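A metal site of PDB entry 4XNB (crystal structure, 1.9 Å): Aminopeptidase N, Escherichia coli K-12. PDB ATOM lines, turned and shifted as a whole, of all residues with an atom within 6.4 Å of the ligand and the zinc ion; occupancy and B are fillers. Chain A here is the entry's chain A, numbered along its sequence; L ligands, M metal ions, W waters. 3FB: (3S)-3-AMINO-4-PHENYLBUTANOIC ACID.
The side-chain hydroxyl of Tyr 377 sits close to an oxygen (O) of the ligand. The side-chain carboxylate of Glu 294 lies close to an oxygen (OXT) of the ligand, at 2.6 Å. OE1 of Glu 117 lies within salt-bridge range of N of the ligand (2.7 Å). N of the ligand is in salt-bridge range of OE1 of Glu 260 (2.7 Å). The side-chain amino group (NZ) of Lys 315 sits close to a nitrogen (N) of the ligand (3.4 Å).
The side-chain hydroxyl (OH) of Tyr 377 sits close to the side-chain carboxylate (OE2) of Glu 316. The side-chain carboxylate (OE1) of Glu 294 lies within hydrogen-bond range of the backbone NH (N) of Glu 260, at 3.4 Å. NE2 of Gln 115 lies within hydrogen-bond range of O of Glu 117 (3.1 Å). NZ of Lys 315 lies within salt-bridge range of OE2 of Glu 117 (2.7 Å). The side-chain carboxylate of Glu 117 sits at hydrogen-bond distance from the side-chain hydroxyl of Tyr 372, 2.7 Å away. OE2 of Glu 260 lies within salt-bridge range of NZ of Lys 315 (2.9 Å). SD of Met 259 sits at hydrogen-bond distance from NE2 of Gln 115. OG1 of Thr 319 lies within hydrogen-bond range of O of Lys 315.
NE2 of Gln 115 touches CE2 of the ligand, 3.3 Å away. Phe 254 touches the ligand. CG of Met 256 touches CH of the ligand, at 3.4 Å. Ala 258 touches the ligand (O to CCC, 3.1 Å). Met 259 touches the ligand (SD to CA, 3.6 Å). Tyr 372 touches the ligand (CE2 to CB, 3.7 Å). 14 residues have an atom within 4 Å of the ligand: Gln 115, Glu 117, Phe 254, Met 256, Ala 258, Met 259, Glu 260, His 293, Glu 294, His 297, Lys 315, Glu 316, Tyr 372 and Tyr 377.
Merely in contact with the zinc ion: Tyr 377 (3.9 Å). Within 4 Å of the zinc ion: His 293, His 297, Glu 316 and Tyr 377. Along chain A the residues within 4 Å of the zinc ion span positions 293 to 377.
The zinc ion is bound by the side-chain carboxylate of Glu 316, an oxygen (O) of the ligand, a ring nitrogen (NE2) of His 293 and a ring nitrogen (NE2) of His 297. Slightly farther from the zinc ion lies OXT of the ligand (2.6 Å). Slightly farther from the zinc ion lies OE2 of Glu 316 (2.8 Å).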
ATOM      1  N   GLN A 115      18.609  30.098  -0.067  1.00  0.00           N
ATOM      2  CA  GLN A 115      19.100  29.746   1.307  1.00  0.00           C
ATOM      3  C   GLN A 115      20.523  30.185   1.405  1.00  0.00           C
ATOM      4  O   GLN A 115      21.390  29.712   0.615  1.00  0.00           O
ATOM      5  CB  GLN A 115      18.955  28.214   1.516  1.00  0.00           C
ATOM      6  CG  GLN A 115      19.568  27.732   2.826  1.00  0.00           C
ATOM      7  CD  GLN A 115      18.989  28.469   4.017  1.00  0.00           C
ATOM      8  OE1 GLN A 115      17.785  28.777   4.046  1.00  0.00           O
ATOM      9  NE2 GLN A 115      19.812  28.760   4.993  1.00  0.00           N
ATOM     10  N   GLU A 117      22.210  30.885   4.711  1.00  0.00           N
ATOM     11  CA  GLU A 117      22.990  30.437   5.880  1.00  0.00           C
ATOM     12  C   GLU A 117      23.585  29.059   5.566  1.00  0.00           C
ATOM     13  O   GLU A 117      22.875  28.229   5.048  1.00  0.00           O
ATOM     14  CB  GLU A 117      22.156  30.366   7.149  1.00  0.00           C
ATOM     15  CG  GLU A 117      22.998  30.159   8.387  1.00  0.00           C
ATOM     16  CD  GLU A 117      22.252  30.152   9.703  1.00  0.00           C
ATOM     17  OE1 GLU A 117      21.058  30.531   9.704  1.00  0.00           O
ATOM     18  OE2 GLU A 117      22.870  29.826  10.748  1.00  0.00           O
ATOM     19  N   ALA A 118      24.876  28.802   5.876  1.00  0.00           N
ATOM     20  CA  ALA A 118      25.818  29.744   6.496  1.00  0.00           C
ATOM     21  C   ALA A 118      26.504  30.648   5.457  1.00  0.00           C
ATOM     22  O   ALA A 118      26.601  31.893   5.644  1.00  0.00           O
ATOM     23  CB  ALA A 118      26.908  28.982   7.303  1.00  0.00           C
ATOM     24  N   TYR A 181      23.895  36.282   5.511  1.00  0.00           N
ATOM     25  CA  TYR A 181      23.203  35.018   5.654  1.00  0.00           C
ATOM     26  C   TYR A 181      21.714  35.170   5.887  1.00  0.00           C
ATOM     27  O   TYR A 181      20.962  34.195   5.678  1.00  0.00           O
ATOM     28  CB  TYR A 181      23.834  34.114   6.691  1.00  0.00           C
ATOM     29  CG  TYR A 181      23.455  34.419   8.139  1.00  0.00           C
ATOM     30  CD1 TYR A 181      22.384  33.795   8.730  1.00  0.00           C
ATOM     31  CD2 TYR A 181      24.266  35.253   8.955  1.00  0.00           C
ATOM     32  CE1 TYR A 181      22.034  34.056  10.041  1.00  0.00           C
ATOM     33  CE2 TYR A 181      23.944  35.466  10.305  1.00  0.00           C
ATOM     34  CZ  TYR A 181      22.787  34.889  10.822  1.00  0.00           C
ATOM     35  OH  TYR A 181      22.429  35.137  12.126  1.00  0.00           O
ATOM     36  N   PHE A 254      13.965  21.888   0.377  1.00  0.00           N
ATOM     37  CA  PHE A 254      14.691  22.594   1.389  1.00  0.00           C
ATOM     38  C   PHE A 254      15.542  21.588   2.177  1.00  0.00           C
ATOM     39  O   PHE A 254      15.030  20.539   2.569  1.00  0.00           O
ATOM     40  CB  PHE A 254      13.660  23.268   2.335  1.00  0.00           C
ATOM     41  CG  PHE A 254      14.229  24.409   3.104  1.00  0.00           C
ATOM     42  CD1 PHE A 254      14.540  25.603   2.441  1.00  0.00           C
ATOM     43  CD2 PHE A 254      14.522  24.276   4.510  1.00  0.00           C
ATOM     44  CE1 PHE A 254      15.071  26.662   3.120  1.00  0.00           C
ATOM     45  CE2 PHE A 254      15.104  25.340   5.193  1.00  0.00           C
ATOM     46  CZ  PHE A 254      15.357  26.544   4.502  1.00  0.00           C
ATOM     47  N   ASN A 255      16.804  21.933   2.429  1.00  0.00           N
ATOM     48  CA  ASN A 255      17.711  21.054   3.098  1.00  0.00           C
ATOM     49  C   ASN A 255      17.533  20.861   4.592  1.00  0.00           C
ATOM     50  O   ASN A 255      17.881  19.803   5.097  1.00  0.00           O
ATOM     51  CB  ASN A 255      19.173  21.437   2.791  1.00  0.00           C
ATOM     52  CG  ASN A 255      19.554  21.083   1.354  1.00  0.00           C
ATOM     53  OD1 ASN A 255      18.922  20.212   0.693  1.00  0.00           O
ATOM     54  ND2 ASN A 255      20.634  21.716   0.895  1.00  0.00           N
ATOM     55  N   MET A 256      16.981  21.859   5.293  1.00  0.00           N
ATOM     56  CA  MET A 256      16.732  21.724   6.750  1.00  0.00           C
ATOM     57  C   MET A 256      15.295  21.939   7.065  1.00  0.00           C
ATOM     58  O   MET A 256      14.432  21.592   6.273  1.00  0.00           O
ATOM     59  CB  MET A 256      17.672  22.685   7.510  1.00  0.00           C
ATOM     60  CG  MET A 256      19.120  22.430   7.141  1.00  0.00           C
ATOM     61  SD  MET A 256      20.103  21.908   8.564  1.00  0.00           S
ATOM     62  CE  MET A 256      19.536  23.092   9.863  1.00  0.00           C
ATOM     63  N   GLY A 257      14.991  22.511   8.193  1.00  0.00           N
ATOM     64  CA  GLY A 257      13.621  22.693   8.623  1.00  0.00           C
ATOM     65  C   GLY A 257      13.101  24.059   8.187  1.00  0.00           C
ATOM     66  O   GLY A 257      12.001  24.155   7.686  1.00  0.00           O
ATOM     67  N   ALA A 258      13.839  25.109   8.472  1.00  0.00           N
ATOM     68  CA  ALA A 258      13.306  26.442   8.097  1.00  0.00           C
ATOM     69  C   ALA A 258      14.445  27.425   8.272  1.00  0.00           C
ATOM     70  O   ALA A 258      15.511  27.023   8.663  1.00  0.00           O
ATOM     71  CB  ALA A 258      12.067  26.822   8.900  1.00  0.00           C
ATOM     72  N   MET A 259      14.220  28.713   8.008  1.00  0.00           N
ATOM     73  CA  MET A 259      15.264  29.709   8.066  1.00  0.00           C
ATOM     74  C   MET A 259      14.728  31.096   8.444  1.00  0.00           C
ATOM     75  O   MET A 259      13.744  31.541   7.857  1.00  0.00           O
ATOM     76  CB  MET A 259      15.963  29.734   6.740  1.00  0.00           C
ATOM     77  CG  MET A 259      16.995  30.833   6.547  1.00  0.00           C
ATOM     78  SD  MET A 259      18.406  30.537   7.723  1.00  0.00           S
ATOM     79  CE  MET A 259      18.926  32.201   8.082  1.00  0.00           C
ATOM     80  N   GLU A 260      15.411  31.754   9.378  1.00  0.00           N
ATOM     81  CA  GLU A 260      14.923  32.948  10.035  1.00  0.00           C
ATOM     82  C   GLU A 260      15.233  34.257   9.272  1.00  0.00           C
ATOM     83  O   GLU A 260      15.460  35.265   9.925  1.00  0.00           O
ATOM     84  CB  GLU A 260      15.487  33.071  11.422  1.00  0.00           C
ATOM     85  CG  GLU A 260      17.009  33.278  11.554  1.00  0.00           C
ATOM     86  CD  GLU A 260      17.870  31.976  11.626  1.00  0.00           C
ATOM     87  OE1 GLU A 260      17.418  30.883  11.195  1.00  0.00           O
ATOM     88  OE2 GLU A 260      19.056  32.113  12.082  1.00  0.00           O
ATOM     89  N   HIS A 293      10.533  28.728  16.816  1.00  0.00           N
ATOM     90  CA  HIS A 293      11.974  28.812  16.666  1.00  0.00           C
ATOM     91  C   HIS A 293      12.411  29.925  15.719  1.00  0.00           C
ATOM     92  O   HIS A 293      13.239  30.776  16.094  1.00  0.00           O
ATOM     93  CB  HIS A 293      12.512  27.426  16.185  1.00  0.00           C
ATOM     94  CG  HIS A 293      13.998  27.346  16.152  1.00  0.00           C
ATOM     95  ND1 HIS A 293      14.749  26.885  17.193  1.00  0.00           N
ATOM     96  CD2 HIS A 293      14.876  27.728  15.196  1.00  0.00           C
ATOM     97  CE1 HIS A 293      16.035  27.009  16.916  1.00  0.00           C
ATOM     98  NE2 HIS A 293      16.136  27.512  15.687  1.00  0.00           N
ATOM     99  N   GLU A 294      11.926  29.928  14.479  1.00  0.00           N
ATOM    100  CA  GLU A 294      12.348  30.961  13.521  1.00  0.00           C
ATOM    101  C   GLU A 294      11.957  32.361  14.035  1.00  0.00           C
ATOM    102  O   GLU A 294      12.689  33.294  13.874  1.00  0.00           O
ATOM    103  CB  GLU A 294      11.861  30.691  12.089  1.00  0.00           C
ATOM    104  CG  GLU A 294      12.067  29.236  11.640  1.00  0.00           C
ATOM    105  CD  GLU A 294      13.502  28.705  11.825  1.00  0.00           C
ATOM    106  OE1 GLU A 294      14.430  29.500  11.664  1.00  0.00           O
ATOM    107  OE2 GLU A 294      13.668  27.494  12.025  1.00  0.00           O
ATOM    108  N   HIS A 297      14.350  33.654  16.695  1.00  0.00           N
ATOM    109  CA  HIS A 297      15.596  34.132  16.151  1.00  0.00           C
ATOM    110  C   HIS A 297      15.562  35.619  15.798  1.00  0.00           C
ATOM    111  O   HIS A 297      16.585  36.215  15.633  1.00  0.00           O
ATOM    112  CB  HIS A 297      15.918  33.388  14.836  1.00  0.00           C
ATOM    113  CG  HIS A 297      16.747  32.147  14.990  1.00  0.00           C
ATOM    114  ND1 HIS A 297      17.918  32.124  15.703  1.00  0.00           N
ATOM    115  CD2 HIS A 297      16.603  30.902  14.457  1.00  0.00           C
ATOM    116  CE1 HIS A 297      18.473  30.935  15.586  1.00  0.00           C
ATOM    117  NE2 HIS A 297      17.694  30.199  14.846  1.00  0.00           N
ATOM    118  N   LEU A 312      28.029  29.878  16.439  1.00  0.00           N
ATOM    119  CA  LEU A 312      26.725  29.482  16.049  1.00  0.00           C
ATOM    120  C   LEU A 312      25.784  29.175  17.231  1.00  0.00           C
ATOM    121  O   LEU A 312      24.611  29.587  17.211  1.00  0.00           O
ATOM    122  CB  LEU A 312      26.784  28.260  15.084  1.00  0.00           C
ATOM    123  CG  LEU A 312      25.442  27.728  14.596  1.00  0.00           C
ATOM    124  CD1 LEU A 312      24.668  28.791  13.785  1.00  0.00           C
ATOM    125  CD2 LEU A 312      25.622  26.534  13.767  1.00  0.00           C
ATOM    126  N   LYS A 315      23.316  31.803  18.943  1.00  0.00           N
ATOM    127  CA  LYS A 315      21.964  31.896  18.482  1.00  0.00           C
ATOM    128  C   LYS A 315      21.217  30.563  18.514  1.00  0.00           C
ATOM    129  O   LYS A 315      20.027  30.559  18.844  1.00  0.00           O
ATOM    130  CB  LYS A 315      21.842  32.596  17.107  1.00  0.00           C
ATOM    131  CG  LYS A 315      22.349  31.835  15.888  1.00  0.00           C
ATOM    132  CD  LYS A 315      22.183  32.658  14.602  1.00  0.00           C
ATOM    133  CE  LYS A 315      22.544  31.965  13.280  1.00  0.00           C
ATOM    134  NZ  LYS A 315      21.620  30.952  12.799  1.00  0.00           N
ATOM    135  N   GLU A 316      21.870  29.442  18.204  1.00  0.00           N
ATOM    136  CA  GLU A 316      21.134  28.200  18.109  1.00  0.00           C
ATOM    137  C   GLU A 316      20.794  27.570  19.477  1.00  0.00           C
ATOM    138  O   GLU A 316      19.670  27.125  19.679  1.00  0.00           O
ATOM    139  CB  GLU A 316      21.755  27.206  17.140  1.00  0.00           C
ATOM    140  CG  GLU A 316      21.855  27.695  15.698  1.00  0.00           C
ATOM    141  CD  GLU A 316      20.533  28.075  15.112  1.00  0.00           C
ATOM    142  OE1 GLU A 316      19.521  27.714  15.726  1.00  0.00           O
ATOM    143  OE2 GLU A 316      20.535  28.809  14.098  1.00  0.00           O
ATOM    144  N   THR A 319      18.142  29.939  20.983  1.00  0.00           N
ATOM    145  CA  THR A 319      16.839  29.868  20.287  1.00  0.00           C
ATOM    146  C   THR A 319      16.144  28.507  20.475  1.00  0.00           C
ATOM    147  O   THR A 319      14.944  28.434  20.585  1.00  0.00           O
ATOM    148  CB  THR A 319      16.956  30.303  18.814  1.00  0.00           C
ATOM    149  OG1 THR A 319      17.586  31.606  18.782  1.00  0.00           O
ATOM    150  CG2 THR A 319      15.623  30.278  18.120  1.00  0.00           C
ATOM    151  N   VAL A 320      16.926  27.426  20.492  1.00  0.00           N
ATOM    152  CA  VAL A 320      16.354  26.142  20.896  1.00  0.00           C
ATOM    153  C   VAL A 320      15.842  26.160  22.345  1.00  0.00           C
ATOM    154  O   VAL A 320      14.751  25.676  22.625  1.00  0.00           O
ATOM    155  CB  VAL A 320      17.361  24.959  20.758  1.00  0.00           C
ATOM    156  CG1 VAL A 320      16.773  23.706  21.425  1.00  0.00           C
ATOM    157  CG2 VAL A 320      17.731  24.695  19.311  1.00  0.00           C
ATOM    158  N   ASN A 369      28.634  23.864   7.120  1.00  0.00           N
ATOM    159  CA  ASN A 369      27.317  23.197   7.107  1.00  0.00           C
ATOM    160  C   ASN A 369      27.292  21.865   7.813  1.00  0.00           C
ATOM    161  O   ASN A 369      26.195  21.416   8.168  1.00  0.00           O
ATOM    162  CB  ASN A 369      26.778  23.008   5.723  1.00  0.00           C
ATOM    163  CG  ASN A 369      26.395  24.366   5.036  1.00  0.00           C
ATOM    164  OD1 ASN A 369      25.887  25.351   5.673  1.00  0.00           O
ATOM    165  ND2 ASN A 369      26.638  24.389   3.710  1.00  0.00           N
ATOM    166  N   TYR A 372      25.782  22.220  11.962  1.00  0.00           N
ATOM    167  CA  TYR A 372      24.388  22.459  12.391  1.00  0.00           C
ATOM    168  C   TYR A 372      23.935  21.198  13.107  1.00  0.00           C
ATOM    169  O   TYR A 372      23.159  20.439  12.601  1.00  0.00           O
ATOM    170  CB  TYR A 372      23.530  22.843  11.164  1.00  0.00           C
ATOM    171  CG  TYR A 372      23.881  24.269  10.802  1.00  0.00           C
ATOM    172  CD1 TYR A 372      25.027  24.570  10.043  1.00  0.00           C
ATOM    173  CD2 TYR A 372      23.104  25.328  11.224  1.00  0.00           C
ATOM    174  CE1 TYR A 372      25.427  25.896   9.845  1.00  0.00           C
ATOM    175  CE2 TYR A 372      23.489  26.671  11.023  1.00  0.00           C
ATOM    176  CZ  TYR A 372      24.648  26.925  10.274  1.00  0.00           C
ATOM    177  OH  TYR A 372      25.000  28.239  10.084  1.00  0.00           O
ATOM    178  N   TYR A 377      22.975  22.706  18.749  1.00  0.00           N
ATOM    179  CA  TYR A 377      21.537  23.024  19.009  1.00  0.00           C
ATOM    180  C   TYR A 377      21.062  22.487  20.380  1.00  0.00           C
ATOM    181  O   TYR A 377      20.766  23.250  21.306  1.00  0.00           O
ATOM    182  CB  TYR A 377      20.685  22.432  17.891  1.00  0.00           C
ATOM    183  CG  TYR A 377      20.641  23.240  16.636  1.00  0.00           C
ATOM    184  CD1 TYR A 377      21.744  23.399  15.802  1.00  0.00           C
ATOM    185  CD2 TYR A 377      19.397  23.798  16.196  1.00  0.00           C
ATOM    186  CE1 TYR A 377      21.649  24.169  14.624  1.00  0.00           C
ATOM    187  CE2 TYR A 377      19.311  24.527  15.016  1.00  0.00           C
ATOM    188  CZ  TYR A 377      20.428  24.711  14.237  1.00  0.00           C
ATOM    189  OH  TYR A 377      20.308  25.507  13.065  1.00  0.00           O
ATOM    190  N   GLN A 817      25.033  18.634   1.218  1.00  0.00           N
ATOM    191  CA  GLN A 817      24.508  18.800   2.540  1.00  0.00           C
ATOM    192  C   GLN A 817      23.672  17.617   2.990  1.00  0.00           C
ATOM    193  O   GLN A 817      23.791  17.154   4.092  1.00  0.00           O
ATOM    194  CB  GLN A 817      23.668  20.081   2.688  1.00  0.00           C
ATOM    195  CG  GLN A 817      24.585  21.236   2.752  1.00  0.00           C
ATOM    196  CD  GLN A 817      23.817  22.617   2.785  1.00  0.00           C
ATOM    197  OE1 GLN A 817      22.892  22.828   3.562  1.00  0.00           O
ATOM    198  NE2 GLN A 817      24.213  23.490   1.952  1.00  0.00           N
HETATM  199  N   3FB L   1      19.360  29.034  11.112  1.00  0.00           N
HETATM  200  CA  3FB L   1      18.829  27.989  10.202  1.00  0.00           C
HETATM  201  CB  3FB L   1      20.061  27.142   9.741  1.00  0.00           C
HETATM  202  CG  3FB L   1      20.031  26.578   8.359  1.00  0.00           C
HETATM  203  CD1 3FB L   1      21.264  26.194   7.838  1.00  0.00           C
HETATM  204  CE1 3FB L   1      21.246  25.616   6.572  1.00  0.00           C
HETATM  205  CH  3FB L   1      20.104  25.438   5.822  1.00  0.00           C
HETATM  206  CE2 3FB L   1      18.877  25.848   6.356  1.00  0.00           C
HETATM  207  CD2 3FB L   1      18.860  26.396   7.623  1.00  0.00           C
HETATM  208  CCC 3FB L   1      17.792  26.999  10.763  1.00  0.00           C
HETATM  209  C   3FB L   1      17.523  27.400  12.186  1.00  0.00           C
HETATM  210  O   3FB L   1      18.232  27.038  13.105  1.00  0.00           O
HETATM  211  OXT 3FB L   1      16.612  28.270  12.420  1.00  0.00           O
HETATM  212 ZN    ZN M   1      17.854  28.130  14.736  1.00  0.00          ZN
HETATM  213  O   HOH W   1      18.024  24.302   3.575  1.00  0.00           O
